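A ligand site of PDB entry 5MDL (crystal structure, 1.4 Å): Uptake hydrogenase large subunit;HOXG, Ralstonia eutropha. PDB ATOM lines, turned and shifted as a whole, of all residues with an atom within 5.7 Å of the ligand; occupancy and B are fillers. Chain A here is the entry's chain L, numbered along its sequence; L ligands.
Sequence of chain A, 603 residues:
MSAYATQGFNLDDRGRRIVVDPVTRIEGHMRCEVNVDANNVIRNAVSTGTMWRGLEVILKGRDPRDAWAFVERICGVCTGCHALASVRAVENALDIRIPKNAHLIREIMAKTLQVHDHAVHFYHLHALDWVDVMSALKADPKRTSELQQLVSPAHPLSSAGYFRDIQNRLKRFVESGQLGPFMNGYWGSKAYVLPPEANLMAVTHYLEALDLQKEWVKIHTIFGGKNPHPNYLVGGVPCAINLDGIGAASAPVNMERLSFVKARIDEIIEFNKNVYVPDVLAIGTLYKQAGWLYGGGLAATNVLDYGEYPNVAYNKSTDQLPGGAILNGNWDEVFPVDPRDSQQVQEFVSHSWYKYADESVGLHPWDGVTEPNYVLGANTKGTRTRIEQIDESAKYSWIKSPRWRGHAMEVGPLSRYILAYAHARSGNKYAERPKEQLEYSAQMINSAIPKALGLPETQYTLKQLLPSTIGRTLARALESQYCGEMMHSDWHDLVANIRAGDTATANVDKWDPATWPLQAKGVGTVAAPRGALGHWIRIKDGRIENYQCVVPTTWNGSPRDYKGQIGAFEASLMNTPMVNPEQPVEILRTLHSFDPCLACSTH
NI1 of the ligand is bound by SG of Cys 597, 2.2 Å away. The side-chain sulfur (SG) of Cys 75 binds a nickel atom (NI1) of the ligand (2.2 Å). An iron atom (FE1) of the ligand is bound by the side-chain sulfur (SG) of Cys 78 (2.3 Å). SG of Cys 600 is bound to FE1 of the ligand (2.3 Å). N1 of the ligand sits at hydrogen-bond distance from N of Thr 553, 3.0 Å away. A nitrogen (N1) of the ligand is in hydrogen-bond range of the side-chain hydroxyl (OG1) of Thr 553 (2.9 Å). N of Arg 530 lies within hydrogen-bond range of N2 of the ligand, at 2.9 Å. A nitrogen (N2) of the ligand lies within hydrogen-bond range of the guanidinium group (NH1) of Arg 530 (3.4 Å). A ring nitrogen (NE2) of His 82 sits close to an oxygen (O1) of the ligand. SG of Cys 81 sits at hydrogen-bond distance from O1 of the ligand (3.5 Å).
OG1 of Thr 553 sits at hydrogen-bond distance from N of Cys 597. The side-chain sulfur of Cys 597 lies close to the side-chain carboxylate of Glu 27 (3.4 Å). The side-chain sulfur of Cys 75 lies close to the backbone NH of Val 77. The backbone carbonyl oxygen of Cys 78 is in hydrogen-bond range of the side-chain sulfur of Cys 81, at 3.2 Å. NE2 of His 82 lies close to SG of Cys 600. NH2 of Arg 530 is in salt-bridge range of OD1 of Asp 117. The side-chain carboxylate of Asp 595 lies within salt-bridge range of the guanidinium group of Arg 530 (2.8 Å). The side-chain hydroxyl (OG1) of Thr 554 is in hydrogen-bond range of the backbone NH (N) of Val 551 (3.2 Å).
A nitrogen (N2) of the ligand lies close to the backbone nitrogen of Pro 529, at 3.2 Å. Ala 528 touches the ligand. Leu 533 touches the ligand. Val 551 touches the ligand. CD of Pro 552 touches O1 of the ligand, at 3.3 Å. Hydrophobic or aromatic side chains within 4 Å of the ligand: His 82, Ala 528, Pro 529, Leu 533, Val 551 and Pro 552. Within 4 Å of the ligand: Cys 75, Cys 78, Cys 81, His 82, Ala 528, Pro 529, Arg 530, Leu 533, Val 551, Pro 552, Thr 553, Cys 597 and Cys 600.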
ATOM      1  N   GLU A  27      25.615  16.913 -13.257  1.00  0.00           N
ATOM      2  CA  GLU A  27      26.050  17.879 -14.266  1.00  0.00           C
ATOM      3  C   GLU A  27      27.556  17.718 -14.419  1.00  0.00           C
ATOM      4  O   GLU A  27      28.291  17.661 -13.425  1.00  0.00           O
ATOM      5  CB  GLU A  27      25.699  19.314 -13.854  1.00  0.00           C
ATOM      6  CG  GLU A  27      25.927  20.356 -14.955  1.00  0.00           C
ATOM      7  CD  GLU A  27      27.402  20.574 -15.292  1.00  0.00           C
ATOM      8  OE1 GLU A  27      28.241  20.446 -14.381  1.00  0.00           O
ATOM      9  OE2 GLU A  27      27.733  20.898 -16.458  1.00  0.00           O
ATOM     10  N   ILE A  74      29.152  29.442 -16.357  1.00  0.00           N
ATOM     11  CA  ILE A  74      29.750  28.376 -15.565  1.00  0.00           C
ATOM     12  C   ILE A  74      28.793  27.175 -15.520  1.00  0.00           C
ATOM     13  O   ILE A  74      29.225  26.013 -15.570  1.00  0.00           O
ATOM     14  CB  ILE A  74      30.122  28.850 -14.156  1.00  0.00           C
ATOM     15  CG1 ILE A  74      31.331  29.777 -14.235  1.00  0.00           C
ATOM     16  CG2 ILE A  74      30.375  27.669 -13.216  1.00  0.00           C
ATOM     17  CD1 ILE A  74      31.636  30.489 -12.925  1.00  0.00           C
ATOM     18  N   CYS A  75      27.484  27.439 -15.450  1.00  0.00           N
ATOM     19  CA  CYS A  75      26.521  26.374 -15.272  1.00  0.00           C
ATOM     20  C   CYS A  75      25.114  26.708 -15.727  1.00  0.00           C
ATOM     21  O   CYS A  75      24.544  27.722 -15.290  1.00  0.00           O
ATOM     22  CB  CYS A  75      26.481  25.955 -13.823  1.00  0.00           C
ATOM     23  SG  CYS A  75      25.595  24.393 -13.619  1.00  0.00           S
ATOM     24  N   GLY A  76      24.549  25.840 -16.569  1.00  0.00           N
ATOM     25  CA  GLY A  76      23.186  25.970 -17.045  1.00  0.00           C
ATOM     26  C   GLY A  76      22.149  25.254 -16.195  1.00  0.00           C
ATOM     27  O   GLY A  76      20.951  25.391 -16.448  1.00  0.00           O
ATOM     28  N   VAL A  77      22.596  24.475 -15.220  1.00  0.00           N
ATOM     29  CA  VAL A  77      21.693  23.790 -14.306  1.00  0.00           C
ATOM     30  C   VAL A  77      21.370  24.760 -13.179  1.00  0.00           C
ATOM     31  O   VAL A  77      20.199  25.121 -12.967  1.00  0.00           O
ATOM     32  CB  VAL A  77      22.295  22.470 -13.790  1.00  0.00           C
ATOM     33  CG1 VAL A  77      21.357  21.813 -12.785  1.00  0.00           C
ATOM     34  CG2 VAL A  77      22.564  21.511 -14.972  1.00  0.00           C
ATOM     35  N   CYS A  78      22.396  25.236 -12.476  1.00  0.00           N
ATOM     36  CA  CYS A  78      22.191  26.301 -11.466  1.00  0.00           C
ATOM     37  C   CYS A  78      22.214  27.668 -12.142  1.00  0.00           C
ATOM     38  O   CYS A  78      22.944  28.587 -11.741  1.00  0.00           O
ATOM     39  CB  CYS A  78      23.212  26.172 -10.318  1.00  0.00           C
ATOM     40  SG  CYS A  78      24.977  26.274 -10.737  1.00  0.00           S
ATOM     41  N   CYS A  81      22.572  31.730 -10.730  1.00  0.00           N
ATOM     42  CA  CYS A  81      23.141  31.977  -9.396  1.00  0.00           C
ATOM     43  C   CYS A  81      24.505  32.641  -9.486  1.00  0.00           C
ATOM     44  O   CYS A  81      24.842  33.472  -8.663  1.00  0.00           O
ATOM     45  CB  CYS A  81      23.159  30.741  -8.497  1.00  0.00           C
ATOM     46  SG  CYS A  81      24.324  29.454  -8.933  1.00  0.00           S
ATOM     47  N   HIS A  82      25.280  32.270 -10.507  1.00  0.00           N
ATOM     48  CA  HIS A  82      26.562  32.919 -10.763  1.00  0.00           C
ATOM     49  C   HIS A  82      26.409  34.361 -11.225  1.00  0.00           C
ATOM     50  O   HIS A  82      27.225  35.212 -10.889  1.00  0.00           O
ATOM     51  CB  HIS A  82      27.355  32.121 -11.802  1.00  0.00           C
ATOM     52  CG  HIS A  82      27.875  30.823 -11.276  1.00  0.00           C
ATOM     53  ND1 HIS A  82      28.893  30.756 -10.348  1.00  0.00           N
ATOM     54  CD2 HIS A  82      27.502  29.544 -11.516  1.00  0.00           C
ATOM     55  CE1 HIS A  82      29.131  29.487 -10.061  1.00  0.00           C
ATOM     56  NE2 HIS A  82      28.293  28.734 -10.750  1.00  0.00           N
ATOM     57  N   ASP A 117      15.746  23.551  -9.601  1.00  0.00           N
ATOM     58  CA  ASP A 117      16.968  22.758  -9.508  1.00  0.00           C
ATOM     59  C   ASP A 117      16.751  21.580  -8.553  1.00  0.00           C
ATOM     60  O   ASP A 117      17.034  20.432  -8.897  1.00  0.00           O
ATOM     61  CB  ASP A 117      18.103  23.677  -9.052  1.00  0.00           C
ATOM     62  CG  ASP A 117      19.458  23.234  -9.477  1.00  0.00           C
ATOM     63  OD1 ASP A 117      19.670  22.015  -9.610  1.00  0.00           O
ATOM     64  OD2 ASP A 117      20.331  24.130  -9.608  1.00  0.00           O
ATOM     65  N   ALA A 528      23.494  29.280  -3.120  1.00  0.00           N
ATOM     66  CA  ALA A 528      23.123  28.605  -4.348  1.00  0.00           C
ATOM     67  C   ALA A 528      22.485  27.248  -4.023  1.00  0.00           C
ATOM     68  O   ALA A 528      22.625  26.757  -2.906  1.00  0.00           O
ATOM     69  CB  ALA A 528      24.353  28.427  -5.226  1.00  0.00           C
ATOM     70  N   PRO A 529      21.798  26.636  -4.997  1.00  0.00           N
ATOM     71  CA  PRO A 529      21.146  25.344  -4.702  1.00  0.00           C
ATOM     72  C   PRO A 529      22.006  24.263  -4.041  1.00  0.00           C
ATOM     73  O   PRO A 529      21.519  23.540  -3.202  1.00  0.00           O
ATOM     74  CB  PRO A 529      20.624  24.912  -6.056  1.00  0.00           C
ATOM     75  CG  PRO A 529      20.327  26.200  -6.756  1.00  0.00           C
ATOM     76  CD  PRO A 529      21.397  27.150  -6.316  1.00  0.00           C
ATOM     77  N   ARG A 530      23.291  24.208  -4.366  1.00  0.00           N
ATOM     78  CA  ARG A 530      24.168  23.176  -3.822  1.00  0.00           C
ATOM     79  C   ARG A 530      25.000  23.622  -2.622  1.00  0.00           C
ATOM     80  O   ARG A 530      25.758  22.825  -2.082  1.00  0.00           O
ATOM     81  CB  ARG A 530      25.085  22.647  -4.938  1.00  0.00           C
ATOM     82  CG  ARG A 530      24.336  21.781  -5.928  1.00  0.00           C
ATOM     83  CD  ARG A 530      24.915  21.824  -7.335  1.00  0.00           C
ATOM     84  NE  ARG A 530      24.013  21.151  -8.264  1.00  0.00           N
ATOM     85  CZ  ARG A 530      22.968  21.714  -8.853  1.00  0.00           C
ATOM     86  NH1 ARG A 530      22.703  23.014  -8.712  1.00  0.00           N
ATOM     87  NH2 ARG A 530      22.203  20.968  -9.645  1.00  0.00           N
ATOM     88  N   GLY A 531      24.878  24.891  -2.211  1.00  0.00           N
ATOM     89  CA  GLY A 531      25.583  25.381  -1.017  1.00  0.00           C
ATOM     90  C   GLY A 531      26.113  26.782  -1.163  1.00  0.00           C
ATOM     91  O   GLY A 531      25.503  27.643  -1.793  1.00  0.00           O
ATOM     92  N   LEU A 533      28.129  29.775  -2.350  1.00  0.00           N
ATOM     93  CA  LEU A 533      28.778  30.307  -3.545  1.00  0.00           C
ATOM     94  C   LEU A 533      29.344  31.691  -3.248  1.00  0.00           C
ATOM     95  O   LEU A 533      28.644  32.542  -2.680  1.00  0.00           O
ATOM     96  CB  LEU A 533      27.761  30.458  -4.684  1.00  0.00           C
ATOM     97  CG  LEU A 533      28.255  31.210  -5.939  1.00  0.00           C
ATOM     98  CD1 LEU A 533      29.413  30.491  -6.613  1.00  0.00           C
ATOM     99  CD2 LEU A 533      27.103  31.380  -6.936  1.00  0.00           C
ATOM    100  N   VAL A 551      32.858  27.689  -5.448  1.00  0.00           N
ATOM    101  CA  VAL A 551      31.510  27.284  -5.826  1.00  0.00           C
ATOM    102  C   VAL A 551      31.122  26.091  -4.910  1.00  0.00           C
ATOM    103  O   VAL A 551      32.009  25.435  -4.358  1.00  0.00           O
ATOM    104  CB  VAL A 551      31.505  26.987  -7.358  1.00  0.00           C
ATOM    105  CG1 VAL A 551      30.142  26.709  -7.910  1.00  0.00           C
ATOM    106  CG2 VAL A 551      32.105  28.162  -8.124  1.00  0.00           C
ATOM    107  N   PRO A 552      29.822  25.857  -4.664  1.00  0.00           N
ATOM    108  CA  PRO A 552      29.472  24.840  -3.670  1.00  0.00           C
ATOM    109  C   PRO A 552      30.075  23.464  -3.923  1.00  0.00           C
ATOM    110  O   PRO A 552      30.612  22.866  -3.003  1.00  0.00           O
ATOM    111  CB  PRO A 552      27.963  24.790  -3.745  1.00  0.00           C
ATOM    112  CG  PRO A 552      27.559  26.157  -4.179  1.00  0.00           C
ATOM    113  CD  PRO A 552      28.638  26.642  -5.079  1.00  0.00           C
ATOM    114  N   THR A 553      30.052  22.987  -5.169  1.00  0.00           N
ATOM    115  CA  THR A 553      30.627  21.688  -5.495  1.00  0.00           C
ATOM    116  C   THR A 553      32.165  21.730  -5.447  1.00  0.00           C
ATOM    117  O   THR A 553      32.810  20.679  -5.287  1.00  0.00           O
ATOM    118  CB  THR A 553      30.055  21.129  -6.807  1.00  0.00           C
ATOM    119  OG1 THR A 553      28.631  21.088  -6.700  1.00  0.00           O
ATOM    120  CG2 THR A 553      30.542  19.702  -7.065  1.00  0.00           C
ATOM    121  N   THR A 554      32.769  22.925  -5.508  1.00  0.00           N
ATOM    122  CA  THR A 554      34.198  23.041  -5.202  1.00  0.00           C
ATOM    123  C   THR A 554      34.461  22.598  -3.752  1.00  0.00           C
ATOM    124  O   THR A 554      35.366  21.785  -3.499  1.00  0.00           O
ATOM    125  CB  THR A 554      34.756  24.467  -5.400  1.00  0.00           C
ATOM    126  OG1 THR A 554      34.246  25.052  -6.623  1.00  0.00           O
ATOM    127  CG2 THR A 554      36.276  24.433  -5.458  1.00  0.00           C
ATOM    128  N   ASP A 595      24.050  16.448  -5.041  1.00  0.00           N
ATOM    129  CA  ASP A 595      23.701  17.090  -6.290  1.00  0.00           C
ATOM    130  C   ASP A 595      24.956  17.678  -6.976  1.00  0.00           C
ATOM    131  O   ASP A 595      25.069  18.872  -7.215  1.00  0.00           O
ATOM    132  CB  ASP A 595      22.610  18.129  -5.952  1.00  0.00           C
ATOM    133  CG  ASP A 595      22.110  18.882  -7.121  1.00  0.00           C
ATOM    134  OD1 ASP A 595      22.262  18.478  -8.308  1.00  0.00           O
ATOM    135  OD2 ASP A 595      21.519  19.961  -6.849  1.00  0.00           O
ATOM    136  N   CYS A 597      27.585  19.313  -9.216  1.00  0.00           N
ATOM    137  CA  CYS A 597      27.676  20.090 -10.428  1.00  0.00           C
ATOM    138  C   CYS A 597      29.134  20.299 -10.741  1.00  0.00           C
ATOM    139  O   CYS A 597      29.811  21.111 -10.121  1.00  0.00           O
ATOM    140  CB  CYS A 597      26.965  21.431 -10.282  1.00  0.00           C
ATOM    141  SG  CYS A 597      26.739  22.252 -11.872  1.00  0.00           S
ATOM    142  N   CYS A 600      30.281  23.637 -12.429  1.00  0.00           N
ATOM    143  CA  CYS A 600      30.374  24.588 -11.326  1.00  0.00           C
ATOM    144  C   CYS A 600      31.658  24.435 -10.532  1.00  0.00           C
ATOM    145  O   CYS A 600      32.321  25.408 -10.199  1.00  0.00           O
ATOM    146  CB  CYS A 600      29.205  24.394 -10.365  1.00  0.00           C
ATOM    147  SG  CYS A 600      27.850  25.520 -10.679  1.00  0.00           S
ATOM    148  N   SER A 601      31.991  23.197 -10.194  1.00  0.00           N
ATOM    149  CA  SER A 601      33.072  22.948  -9.245  1.00  0.00           C
ATOM    150  C   SER A 601      34.415  23.424  -9.764  1.00  0.00           C
ATOM    151  O   SER A 601      35.256  23.841  -8.975  1.00  0.00           O
ATOM    152  CB  SER A 601      33.152  21.461  -8.893  1.00  0.00           C
ATOM    153  OG  SER A 601      33.681  20.654  -9.933  1.00  0.00           O
HETATM  154 FE1  LIG L   1      26.265  25.512  -8.954  1.00  0.00          FE
HETATM  155 NI1  LIG L   1      25.801  24.169 -11.448  1.00  0.00          NI
HETATM  156  C1  LIG L   1      26.849  27.185  -8.198  1.00  0.00           C
HETATM  157  O1  LIG L   1      27.324  28.328  -7.651  1.00  0.00           O
HETATM  158  C2  LIG L   1      27.325  24.511  -7.855  1.00  0.00           C
HETATM  159  N1  LIG L   1      28.031  23.890  -7.185  1.00  0.00           N
HETATM  160  C3  LIG L   1      24.936  25.445  -7.693  1.00  0.00           C
HETATM  161  N2  LIG L   1      24.107  25.459  -6.895  1.00  0.00           N
HETATM  162  O2  LIG L   1      25.523  23.682  -9.715  1.00  0.00           O
